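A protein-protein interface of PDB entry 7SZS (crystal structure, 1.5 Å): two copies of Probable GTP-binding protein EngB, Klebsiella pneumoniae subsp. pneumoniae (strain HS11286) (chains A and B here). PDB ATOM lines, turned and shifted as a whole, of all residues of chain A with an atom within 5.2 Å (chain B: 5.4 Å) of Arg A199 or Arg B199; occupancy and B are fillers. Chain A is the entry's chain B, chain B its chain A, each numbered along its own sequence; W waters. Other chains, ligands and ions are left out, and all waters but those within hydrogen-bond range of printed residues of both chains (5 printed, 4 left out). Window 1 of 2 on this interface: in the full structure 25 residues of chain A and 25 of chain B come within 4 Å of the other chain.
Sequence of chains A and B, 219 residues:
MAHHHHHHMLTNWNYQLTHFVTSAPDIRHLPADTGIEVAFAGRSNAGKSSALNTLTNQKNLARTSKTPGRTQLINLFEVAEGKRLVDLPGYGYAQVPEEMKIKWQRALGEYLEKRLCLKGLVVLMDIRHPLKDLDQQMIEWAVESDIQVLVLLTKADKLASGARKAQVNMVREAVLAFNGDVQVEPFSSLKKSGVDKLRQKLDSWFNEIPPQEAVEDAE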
ATOM      1  N   ASN A  12      -9.771 -15.379  10.422  1.00  0.00           N
ATOM      2  CA  ASN A  12      -8.674 -16.311  10.171  1.00  0.00           C
ATOM      3  C   ASN A  12      -9.290 -17.677   9.912  1.00  0.00           C
ATOM      4  O   ASN A  12      -9.700 -18.378  10.841  1.00  0.00           O
ATOM      5  CB  ASN A  12      -7.708 -16.337  11.352  1.00  0.00           C
ATOM      6  CG  ASN A  12      -7.073 -14.983  11.624  1.00  0.00           C
ATOM      7  OD1 ASN A  12      -6.994 -14.551  12.780  1.00  0.00           O
ATOM      8  ND2 ASN A  12      -6.600 -14.313  10.565  1.00  0.00           N
ATOM      9  N   TYR A  15      -7.610 -23.458   7.577  1.00  0.00           N
ATOM     10  CA  TYR A  15      -7.197 -24.133   6.349  1.00  0.00           C
ATOM     11  C   TYR A  15      -6.981 -25.617   6.564  1.00  0.00           C
ATOM     12  O   TYR A  15      -6.938 -26.370   5.580  1.00  0.00           O
ATOM     13  CB  TYR A  15      -5.937 -23.462   5.767  1.00  0.00           C
ATOM     14  CG  TYR A  15      -6.281 -22.046   5.397  1.00  0.00           C
ATOM     15  CD1 TYR A  15      -7.005 -21.771   4.233  1.00  0.00           C
ATOM     16  CD2 TYR A  15      -5.967 -20.993   6.247  1.00  0.00           C
ATOM     17  CE1 TYR A  15      -7.405 -20.488   3.912  1.00  0.00           C
ATOM     18  CE2 TYR A  15      -6.352 -19.692   5.928  1.00  0.00           C
ATOM     19  CZ  TYR A  15      -7.072 -19.448   4.762  1.00  0.00           C
ATOM     20  OH  TYR A  15      -7.481 -18.177   4.429  1.00  0.00           O
ATOM     21  N   LEU A  55      -0.027 -26.278   4.126  1.00  0.00           N
ATOM     22  CA  LEU A  55      -1.047 -25.314   4.539  1.00  0.00           C
ATOM     23  C   LEU A  55      -2.226 -25.989   5.226  1.00  0.00           C
ATOM     24  O   LEU A  55      -2.749 -25.487   6.232  1.00  0.00           O
ATOM     25  CB  LEU A  55      -1.530 -24.549   3.309  1.00  0.00           C
ATOM     26  CG  LEU A  55      -2.781 -23.698   3.507  1.00  0.00           C
ATOM     27  CD1 LEU A  55      -2.434 -22.503   4.391  1.00  0.00           C
ATOM     28  CD2 LEU A  55      -3.305 -23.248   2.148  1.00  0.00           C
ATOM     29  N   VAL A 195       4.298 -20.482   6.284  1.00  0.00           N
ATOM     30  CA  VAL A 195       2.880 -20.817   6.238  1.00  0.00           C
ATOM     31  C   VAL A 195       2.050 -19.657   6.751  1.00  0.00           C
ATOM     32  O   VAL A 195       0.960 -19.387   6.229  1.00  0.00           O
ATOM     33  CB  VAL A 195       2.598 -22.103   7.035  1.00  0.00           C
ATOM     34  CG1 VAL A 195       1.161 -22.570   6.779  1.00  0.00           C
ATOM     35  CG2 VAL A 195       3.613 -23.198   6.673  1.00  0.00           C
ATOM     36  N   ASP A 196       2.549 -18.953   7.768  1.00  0.00           N
ATOM     37  CA  ASP A 196       1.832 -17.783   8.270  1.00  0.00           C
ATOM     38  C   ASP A 196       1.640 -16.738   7.174  1.00  0.00           C
ATOM     39  O   ASP A 196       0.541 -16.194   7.011  1.00  0.00           O
ATOM     40  CB  ASP A 196       2.555 -17.185   9.481  1.00  0.00           C
ATOM     41  CG  ASP A 196       4.056 -16.906   9.240  1.00  0.00           C
ATOM     42  OD1 ASP A 196       4.661 -17.234   8.180  1.00  0.00           O
ATOM     43  OD2 ASP A 196       4.658 -16.333  10.171  1.00  0.00           O
ATOM     44  N   LYS A 197       2.692 -16.452   6.402  1.00  0.00           N
ATOM     45  CA  LYS A 197       2.572 -15.472   5.322  1.00  0.00           C
ATOM     46  C   LYS A 197       1.514 -15.886   4.308  1.00  0.00           C
ATOM     47  O   LYS A 197       0.762 -15.047   3.795  1.00  0.00           O
ATOM     48  CB  LYS A 197       3.914 -15.289   4.613  1.00  0.00           C
ATOM     49  CG  LYS A 197       5.040 -14.875   5.522  1.00  0.00           C
ATOM     50  CD  LYS A 197       4.823 -13.484   6.060  1.00  0.00           C
ATOM     51  CE  LYS A 197       6.035 -13.020   6.860  1.00  0.00           C
ATOM     52  NZ  LYS A 197       5.889 -11.605   7.291  1.00  0.00           N
ATOM     53  N   LEU A 198       1.459 -17.171   3.983  1.00  0.00           N
ATOM     54  CA  LEU A 198       0.452 -17.664   3.051  1.00  0.00           C
ATOM     55  C   LEU A 198      -0.949 -17.537   3.639  1.00  0.00           C
ATOM     56  O   LEU A 198      -1.872 -17.051   2.971  1.00  0.00           O
ATOM     57  CB  LEU A 198       0.765 -19.117   2.692  1.00  0.00           C
ATOM     58  CG  LEU A 198      -0.243 -19.846   1.803  1.00  0.00           C
ATOM     59  CD1 LEU A 198      -0.466 -19.106   0.484  1.00  0.00           C
ATOM     60  CD2 LEU A 198       0.262 -21.261   1.549  1.00  0.00           C
ATOM     61  N   ARG A 199      -1.124 -17.955   4.896  1.00  0.00           N
ATOM     62  CA  ARG A 199      -2.429 -17.821   5.550  1.00  0.00           C
ATOM     63  C   ARG A 199      -2.889 -16.371   5.590  1.00  0.00           C
ATOM     64  O   ARG A 199      -4.078 -16.086   5.381  1.00  0.00           O
ATOM     65  CB  ARG A 199      -2.372 -18.393   6.966  1.00  0.00           C
ATOM     66  CG  ARG A 199      -2.273 -19.914   7.016  1.00  0.00           C
ATOM     67  CD  ARG A 199      -2.463 -20.414   8.440  1.00  0.00           C
ATOM     68  NE  ARG A 199      -1.422 -19.936   9.352  1.00  0.00           N
ATOM     69  CZ  ARG A 199      -0.620 -20.712  10.071  1.00  0.00           C
ATOM     70  NH1 ARG A 199      -0.629 -22.033   9.944  1.00  0.00           N
ATOM     71  NH2 ARG A 199       0.197 -20.153  10.960  1.00  0.00           N
ATOM     72  N   GLN A 200      -1.973 -15.445   5.884  1.00  0.00           N
ATOM     73  CA  GLN A 200      -2.331 -14.029   5.931  1.00  0.00           C
ATOM     74  C   GLN A 200      -2.846 -13.552   4.583  1.00  0.00           C
ATOM     75  O   GLN A 200      -3.831 -12.803   4.509  1.00  0.00           O
ATOM     76  CB  GLN A 200      -1.122 -13.206   6.357  1.00  0.00           C
ATOM     77  CG  GLN A 200      -0.699 -13.431   7.801  1.00  0.00           C
ATOM     78  CD  GLN A 200       0.746 -13.014   8.056  1.00  0.00           C
ATOM     79  OE1 GLN A 200       1.311 -12.205   7.321  1.00  0.00           O
ATOM     80  NE2 GLN A 200       1.349 -13.578   9.095  1.00  0.00           N
ATOM     81  N   LYS A 201      -2.189 -13.976   3.501  1.00  0.00           N
ATOM     82  CA  LYS A 201      -2.622 -13.554   2.174  1.00  0.00           C
ATOM     83  C   LYS A 201      -3.981 -14.147   1.838  1.00  0.00           C
ATOM     84  O   LYS A 201      -4.868 -13.446   1.333  1.00  0.00           O
ATOM     85  CB  LYS A 201      -1.587 -13.970   1.128  1.00  0.00           C
ATOM     86  CG  LYS A 201      -1.747 -13.237  -0.193  1.00  0.00           C
ATOM     87  CD  LYS A 201      -1.384 -11.753  -0.005  1.00  0.00           C
ATOM     88  CE  LYS A 201      -1.229 -11.032  -1.306  1.00  0.00           C
ATOM     89  NZ  LYS A 201      -0.785  -9.620  -1.068  1.00  0.00           N
ATOM     90  N   LEU A 202      -4.162 -15.443   2.111  1.00  0.00           N
ATOM     91  CA  LEU A 202      -5.444 -16.090   1.861  1.00  0.00           C
ATOM     92  C   LEU A 202      -6.549 -15.437   2.679  1.00  0.00           C
ATOM     93  O   LEU A 202      -7.644 -15.179   2.165  1.00  0.00           O
ATOM     94  CB  LEU A 202      -5.350 -17.583   2.178  1.00  0.00           C
ATOM     95  CG  LEU A 202      -4.349 -18.358   1.337  1.00  0.00           C
ATOM     96  CD1 LEU A 202      -4.323 -19.807   1.797  1.00  0.00           C
ATOM     97  CD2 LEU A 202      -4.695 -18.273  -0.134  1.00  0.00           C
ATOM     98  N   ASP A 203      -6.293 -15.182   3.970  1.00  0.00           N
ATOM     99  CA  ASP A 203      -7.312 -14.528   4.786  1.00  0.00           C
ATOM    100  C   ASP A 203      -7.671 -13.163   4.220  1.00  0.00           C
ATOM    101  O   ASP A 203      -8.843 -12.761   4.243  1.00  0.00           O
ATOM    102  CB  ASP A 203      -6.846 -14.376   6.236  1.00  0.00           C
ATOM    103  CG  ASP A 203      -6.866 -15.696   7.022  1.00  0.00           C
ATOM    104  OD1 ASP A 203      -7.573 -16.648   6.623  1.00  0.00           O
ATOM    105  OD2 ASP A 203      -6.197 -15.748   8.074  1.00  0.00           O
ATOM    106  N   SER A 204      -6.680 -12.428   3.707  1.00  0.00           N
ATOM    107  CA  SER A 204      -6.979 -11.121   3.132  1.00  0.00           C
ATOM    108  C   SER A 204      -7.849 -11.253   1.890  1.00  0.00           C
ATOM    109  O   SER A 204      -8.768 -10.449   1.676  1.00  0.00           O
ATOM    110  CB  SER A 204      -5.684 -10.380   2.805  1.00  0.00           C
ATOM    111  OG  SER A 204      -5.955  -9.195   2.080  1.00  0.00           O
ATOM    112  N   ASN B  12       6.457 -22.525  11.833  1.00  0.00           N
ATOM    113  CA  ASN B  12       5.058 -22.229  12.152  1.00  0.00           C
ATOM    114  C   ASN B  12       4.455 -23.478  12.777  1.00  0.00           C
ATOM    115  O   ASN B  12       4.071 -24.414  12.071  1.00  0.00           O
ATOM    116  CB  ASN B  12       4.282 -21.809  10.910  1.00  0.00           C
ATOM    117  CG  ASN B  12       4.826 -20.550  10.275  1.00  0.00           C
ATOM    118  OD1 ASN B  12       4.955 -20.474   9.053  1.00  0.00           O
ATOM    119  ND2 ASN B  12       5.135 -19.552  11.096  1.00  0.00           N
ATOM    120  N   TRP B  13       4.356 -23.492  14.101  1.00  0.00           N
ATOM    121  CA  TRP B  13       3.884 -24.680  14.795  1.00  0.00           C
ATOM    122  C   TRP B  13       2.404 -24.884  14.533  1.00  0.00           C
ATOM    123  O   TRP B  13       1.668 -23.939  14.240  1.00  0.00           O
ATOM    124  CB  TRP B  13       4.160 -24.567  16.297  1.00  0.00           C
ATOM    125  CG  TRP B  13       5.624 -24.566  16.540  1.00  0.00           C
ATOM    126  CD1 TRP B  13       6.440 -23.479  16.635  1.00  0.00           C
ATOM    127  CD2 TRP B  13       6.472 -25.716  16.639  1.00  0.00           C
ATOM    128  NE1 TRP B  13       7.742 -23.878  16.805  1.00  0.00           N
ATOM    129  CE2 TRP B  13       7.789 -25.249  16.813  1.00  0.00           C
ATOM    130  CE3 TRP B  13       6.242 -27.096  16.599  1.00  0.00           C
ATOM    131  CZ2 TRP B  13       8.877 -26.112  16.955  1.00  0.00           C
ATOM    132  CZ3 TRP B  13       7.323 -27.956  16.745  1.00  0.00           C
ATOM    133  CH2 TRP B  13       8.625 -27.460  16.923  1.00  0.00           C
ATOM    134  N   TYR B  15      -0.790 -25.336  16.073  1.00  0.00           N
ATOM    135  CA  TYR B  15      -1.454 -25.202  17.369  1.00  0.00           C
ATOM    136  C   TYR B  15      -2.729 -26.023  17.459  1.00  0.00           C
ATOM    137  O   TYR B  15      -3.213 -26.251  18.576  1.00  0.00           O
ATOM    138  CB  TYR B  15      -1.715 -23.705  17.676  1.00  0.00           C
ATOM    139  CG  TYR B  15      -0.384 -23.006  17.777  1.00  0.00           C
ATOM    140  CD1 TYR B  15       0.413 -23.181  18.902  1.00  0.00           C
ATOM    141  CD2 TYR B  15       0.127 -22.266  16.709  1.00  0.00           C
ATOM    142  CE1 TYR B  15       1.673 -22.620  18.996  1.00  0.00           C
ATOM    143  CE2 TYR B  15       1.391 -21.686  16.795  1.00  0.00           C
ATOM    144  CZ  TYR B  15       2.158 -21.879  17.937  1.00  0.00           C
ATOM    145  OH  TYR B  15       3.420 -21.334  18.044  1.00  0.00           O
ATOM    146  N   LEU B  55      -7.687 -20.997  19.346  1.00  0.00           N
ATOM    147  CA  LEU B  55      -6.328 -21.240  18.862  1.00  0.00           C
ATOM    148  C   LEU B  55      -6.112 -22.705  18.506  1.00  0.00           C
ATOM    149  O   LEU B  55      -5.476 -23.022  17.490  1.00  0.00           O
ATOM    150  CB  LEU B  55      -5.324 -20.805  19.925  1.00  0.00           C
ATOM    151  CG  LEU B  55      -3.868 -21.208  19.690  1.00  0.00           C
ATOM    152  CD1 LEU B  55      -3.309 -20.397  18.526  1.00  0.00           C
ATOM    153  CD2 LEU B  55      -3.075 -21.000  20.968  1.00  0.00           C
ATOM    154  N   GLY B 194      -7.752 -12.271  14.866  1.00  0.00           N
ATOM    155  CA  GLY B 194      -6.628 -12.071  15.748  1.00  0.00           C
ATOM    156  C   GLY B 194      -5.890 -13.342  16.083  1.00  0.00           C
ATOM    157  O   GLY B 194      -4.884 -13.281  16.799  1.00  0.00           O
ATOM    158  N   VAL B 195      -6.370 -14.490  15.598  1.00  0.00           N
ATOM    159  CA  VAL B 195      -5.675 -15.750  15.843  1.00  0.00           C
ATOM    160  C   VAL B 195      -4.307 -15.719  15.193  1.00  0.00           C
ATOM    161  O   VAL B 195      -3.333 -16.254  15.746  1.00  0.00           O
ATOM    162  CB  VAL B 195      -6.509 -16.931  15.318  1.00  0.00           C
ATOM    163  CG1 VAL B 195      -5.858 -18.257  15.735  1.00  0.00           C
ATOM    164  CG2 VAL B 195      -7.943 -16.822  15.826  1.00  0.00           C
ATOM    165  N   ASP B 196      -4.213 -15.095  14.015  1.00  0.00           N
ATOM    166  CA  ASP B 196      -2.931 -14.985  13.326  1.00  0.00           C
ATOM    167  C   ASP B 196      -1.909 -14.235  14.174  1.00  0.00           C
ATOM    168  O   ASP B 196      -0.762 -14.670  14.312  1.00  0.00           O
ATOM    169  CB  ASP B 196      -3.113 -14.321  11.955  1.00  0.00           C
ATOM    170  CG  ASP B 196      -3.833 -12.949  12.005  1.00  0.00           C
ATOM    171  OD1 ASP B 196      -4.436 -12.514  13.023  1.00  0.00           O
ATOM    172  OD2 ASP B 196      -3.796 -12.271  10.958  1.00  0.00           O
ATOM    173  N   LYS B 197      -2.306 -13.113  14.778  1.00  0.00           N
ATOM    174  CA  LYS B 197      -1.374 -12.370  15.621  1.00  0.00           C
ATOM    175  C   LYS B 197      -0.903 -13.212  16.797  1.00  0.00           C
ATOM    176  O   LYS B 197       0.269 -13.150  17.196  1.00  0.00           O
ATOM    177  CB  LYS B 197      -2.035 -11.094  16.139  1.00  0.00           C
ATOM    178  CG  LYS B 197      -2.553 -10.168  15.063  1.00  0.00           C
ATOM    179  CD  LYS B 197      -1.425  -9.627  14.220  1.00  0.00           C
ATOM    180  CE  LYS B 197      -1.956  -8.640  13.185  1.00  0.00           C
ATOM    181  NZ  LYS B 197      -0.874  -8.056  12.361  1.00  0.00           N
ATOM    182  N   LEU B 198      -1.811 -13.983  17.385  1.00  0.00           N
ATOM    183  CA  LEU B 198      -1.438 -14.847  18.497  1.00  0.00           C
ATOM    184  C   LEU B 198      -0.465 -15.924  18.041  1.00  0.00           C
ATOM    185  O   LEU B 198       0.554 -16.161  18.702  1.00  0.00           O
ATOM    186  CB  LEU B 198      -2.694 -15.456  19.124  1.00  0.00           C
ATOM    187  CG  LEU B 198      -2.464 -16.496  20.221  1.00  0.00           C
ATOM    188  CD1 LEU B 198      -1.631 -15.916  21.352  1.00  0.00           C
ATOM    189  CD2 LEU B 198      -3.818 -16.987  20.741  1.00  0.00           C
ATOM    190  N   ARG B 199      -0.763 -16.590  16.915  1.00  0.00           N
ATOM    191  CA  ARG B 199       0.144 -17.627  16.418  1.00  0.00           C
ATOM    192  C   ARG B 199       1.521 -17.052  16.109  1.00  0.00           C
ATOM    193  O   ARG B 199       2.545 -17.712  16.356  1.00  0.00           O
ATOM    194  CB  ARG B 199      -0.435 -18.302  15.170  1.00  0.00           C
ATOM    195  CG  ARG B 199      -1.663 -19.162  15.423  1.00  0.00           C
ATOM    196  CD  ARG B 199      -2.107 -19.913  14.164  1.00  0.00           C
ATOM    197  NE  ARG B 199      -2.471 -19.044  13.049  1.00  0.00           N
ATOM    198  CZ  ARG B 199      -3.646 -19.072  12.434  1.00  0.00           C
ATOM    199  NH1 ARG B 199      -4.623 -19.869  12.842  1.00  0.00           N
ATOM    200  NH2 ARG B 199      -3.840 -18.299  11.371  1.00  0.00           N
ATOM    201  N   GLN B 200       1.573 -15.842  15.544  1.00  0.00           N
ATOM    202  CA  GLN B 200       2.863 -15.239  15.214  1.00  0.00           C
ATOM    203  C   GLN B 200       3.694 -15.016  16.464  1.00  0.00           C
ATOM    204  O   GLN B 200       4.910 -15.255  16.467  1.00  0.00           O
ATOM    205  CB  GLN B 200       2.658 -13.912  14.488  1.00  0.00           C
ATOM    206  CG  GLN B 200       2.073 -14.035  13.098  1.00  0.00           C
ATOM    207  CD  GLN B 200       1.427 -12.742  12.623  1.00  0.00           C
ATOM    208  OE1 GLN B 200       0.673 -12.734  11.648  1.00  0.00           O
ATOM    209  NE2 GLN B 200       1.715 -11.645  13.317  1.00  0.00           N
ATOM    210  N   LYS B 201       3.053 -14.542  17.534  1.00  0.00           N
ATOM    211  CA  LYS B 201       3.763 -14.321  18.786  1.00  0.00           C
ATOM    212  C   LYS B 201       4.241 -15.639  19.368  1.00  0.00           C
ATOM    213  O   LYS B 201       5.396 -15.760  19.792  1.00  0.00           O
ATOM    214  CB  LYS B 201       2.855 -13.587  19.779  1.00  0.00           C
ATOM    215  CG  LYS B 201       3.627 -12.956  20.936  1.00  0.00           C
ATOM    216  CD  LYS B 201       4.565 -11.878  20.364  1.00  0.00           C
ATOM    217  CE  LYS B 201       5.166 -11.000  21.398  1.00  0.00           C
ATOM    218  NZ  LYS B 201       5.805  -9.824  20.745  1.00  0.00           N
ATOM    219  N   LEU B 202       3.363 -16.647  19.392  1.00  0.00           N
ATOM    220  CA  LEU B 202       3.764 -17.956  19.896  1.00  0.00           C
ATOM    221  C   LEU B 202       4.912 -18.537  19.083  1.00  0.00           C
ATOM    222  O   LEU B 202       5.860 -19.101  19.651  1.00  0.00           O
ATOM    223  CB  LEU B 202       2.576 -18.913  19.883  1.00  0.00           C
ATOM    224  CG  LEU B 202       1.411 -18.481  20.773  1.00  0.00           C
ATOM    225  CD1 LEU B 202       0.258 -19.469  20.635  1.00  0.00           C
ATOM    226  CD2 LEU B 202       1.835 -18.387  22.218  1.00  0.00           C
ATOM    227  N   ASP B 203       4.845 -18.432  17.747  1.00  0.00           N
ATOM    228  CA  ASP B 203       5.936 -18.954  16.927  1.00  0.00           C
ATOM    229  C   ASP B 203       7.243 -18.243  17.250  1.00  0.00           C
ATOM    230  O   ASP B 203       8.314 -18.868  17.272  1.00  0.00           O
ATOM    231  CB  ASP B 203       5.616 -18.800  15.436  1.00  0.00           C
ATOM    232  CG  ASP B 203       4.608 -19.820  14.927  1.00  0.00           C
ATOM    233  OD1 ASP B 203       4.391 -20.858  15.584  1.00  0.00           O
ATOM    234  OD2 ASP B 203       4.050 -19.587  13.838  1.00  0.00           O
ATOM    235  N   SER B 204       7.180 -16.938  17.518  1.00  0.00           N
ATOM    236  CA  SER B 204       8.399 -16.206  17.847  1.00  0.00           C
ATOM    237  C   SER B 204       8.982 -16.686  19.170  1.00  0.00           C
ATOM    238  O   SER B 204      10.208 -16.791  19.310  1.00  0.00           O
ATOM    239  CB  SER B 204       8.114 -14.703  17.883  1.00  0.00           C
ATOM    240  OG  SER B 204       7.495 -14.316  19.098  1.00  0.00           O
HETATM  241  O   HOH W   1       0.127 -23.817  11.989  1.00  0.00           O
HETATM  242  O   HOH W   2       7.380 -18.348   9.032  1.00  0.00           O
HETATM  243  O   HOH W   3      -7.098 -11.386  12.146  1.00  0.00           O
HETATM  244  O   HOH W   4      -5.925 -18.333   9.225  1.00  0.00           O
HETATM  245  O   HOH W   5       1.767 -21.212  13.261  1.00  0.00           O
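Among the printed residues, merely in contact across the chains: Arg A199 with Arg B199 (3.6 Å).
O of Asp A196 sits close to NE2 of Gln A200 (3.4 Å). The side-chain carboxylate (OD2) of Asp A203 lies within hydrogen-bond range of the side-chain amide nitrogen (ND2) of Asn A12, at 2.9 Å. The side-chain amide nitrogen (ND2) of Asn B12 sits at hydrogen-bond distance from the side-chain carboxylate (OD2) of Asp B203, 2.9 Å away.
Asn A12 touches Val B195, and with the chains exchanged Val A195 touches Asn B12. Asn A12 touches Asp B196, and with the chains exchanged Asp A196 touches Asn B12. Arg B199 touches its own counterpart, Arg A199. Gln A200 touches its own counterpart, Gln B200. 13 positions are printed for both chains. Of the 7 pairs that touch across the chains among the printed residues, 6 have their exchanged pair printed and touching as well.
Water W1 bridges the backbone carbonyl oxygen of Trp B13 (2.7 Å) and the guanidinium group of Arg A199 (2.8 Å). Water W4 lies within hydrogen-bond range of OD2 of Asp A203 (2.8 Å) and NH2 of Arg B199 (3.0 Å). Water W5 lies within hydrogen-bond range of OD2 of Asp B203 (2.9 Å), O of Trp B13 (2.9 Å) and NH2 of Arg A199 (3.0 Å). Water W3 lies within hydrogen-bond range of the backbone NH (N) of Gly B194, the side-chain carboxylate (OD1) of Asp B196 and the side-chain amide oxygen (OD1) of Asn A12. Water W2 bridges the side-chain carboxylate of Asp A196 and the side-chain amide oxygen of Asn B12.
N of Gly B194 sits at hydrogen-bond distance from OD1 of Asn A12 (3.2 Å). N of Val B195 lies within hydrogen-bond range of OD1 of Asn A12, 2.9 Å away. OD1 of Asn B12 is in hydrogen-bond range of N of Val A195 (2.8 Å). The side-chain amide oxygen (OE1) of Gln B200 sits at hydrogen-bond distance from the side-chain amide nitrogen (NE2) of Gln A200, 2.8 Å away. OD1 of Asn B12 is in hydrogen-bond range of N of Asp A196 (3.1 Å). The backbone NH (N) of Asp B196 is in hydrogen-bond range of the side-chain amide oxygen (OD1) of Asn A12 (3.1 Å).
Printed residues of chain B within 4 Å of Asn A12: Gly B194 (3.2 Å), Val B195 (2.9 Å) and Asp B196 (3.1 Å). Of the printed residues of chain A, Asn B12 touches Val A195 and Asp A196. Leu B55 touches none of the printed residues of chain A. Of the printed residues of chain A, Asp B196 touches Asn A12 (3.1 Å). Of the printed residues of chain A, Arg B199 touches Arg A199. The nearest printed residue of chain A that does not touch Val B195 is Arg A199 (7.1 Å).
Hydrophobic or aromatic side chains of chain B that line the printed part of chain A: Val B195. Hydrophobic or aromatic side chains of chain A within 4 Å of the printed part of chain B: Val A195. Among the printed residues, no Asp or Glu carboxylate lies within 4 Å of a Lys or Arg side-chain nitrogen of the other chain.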
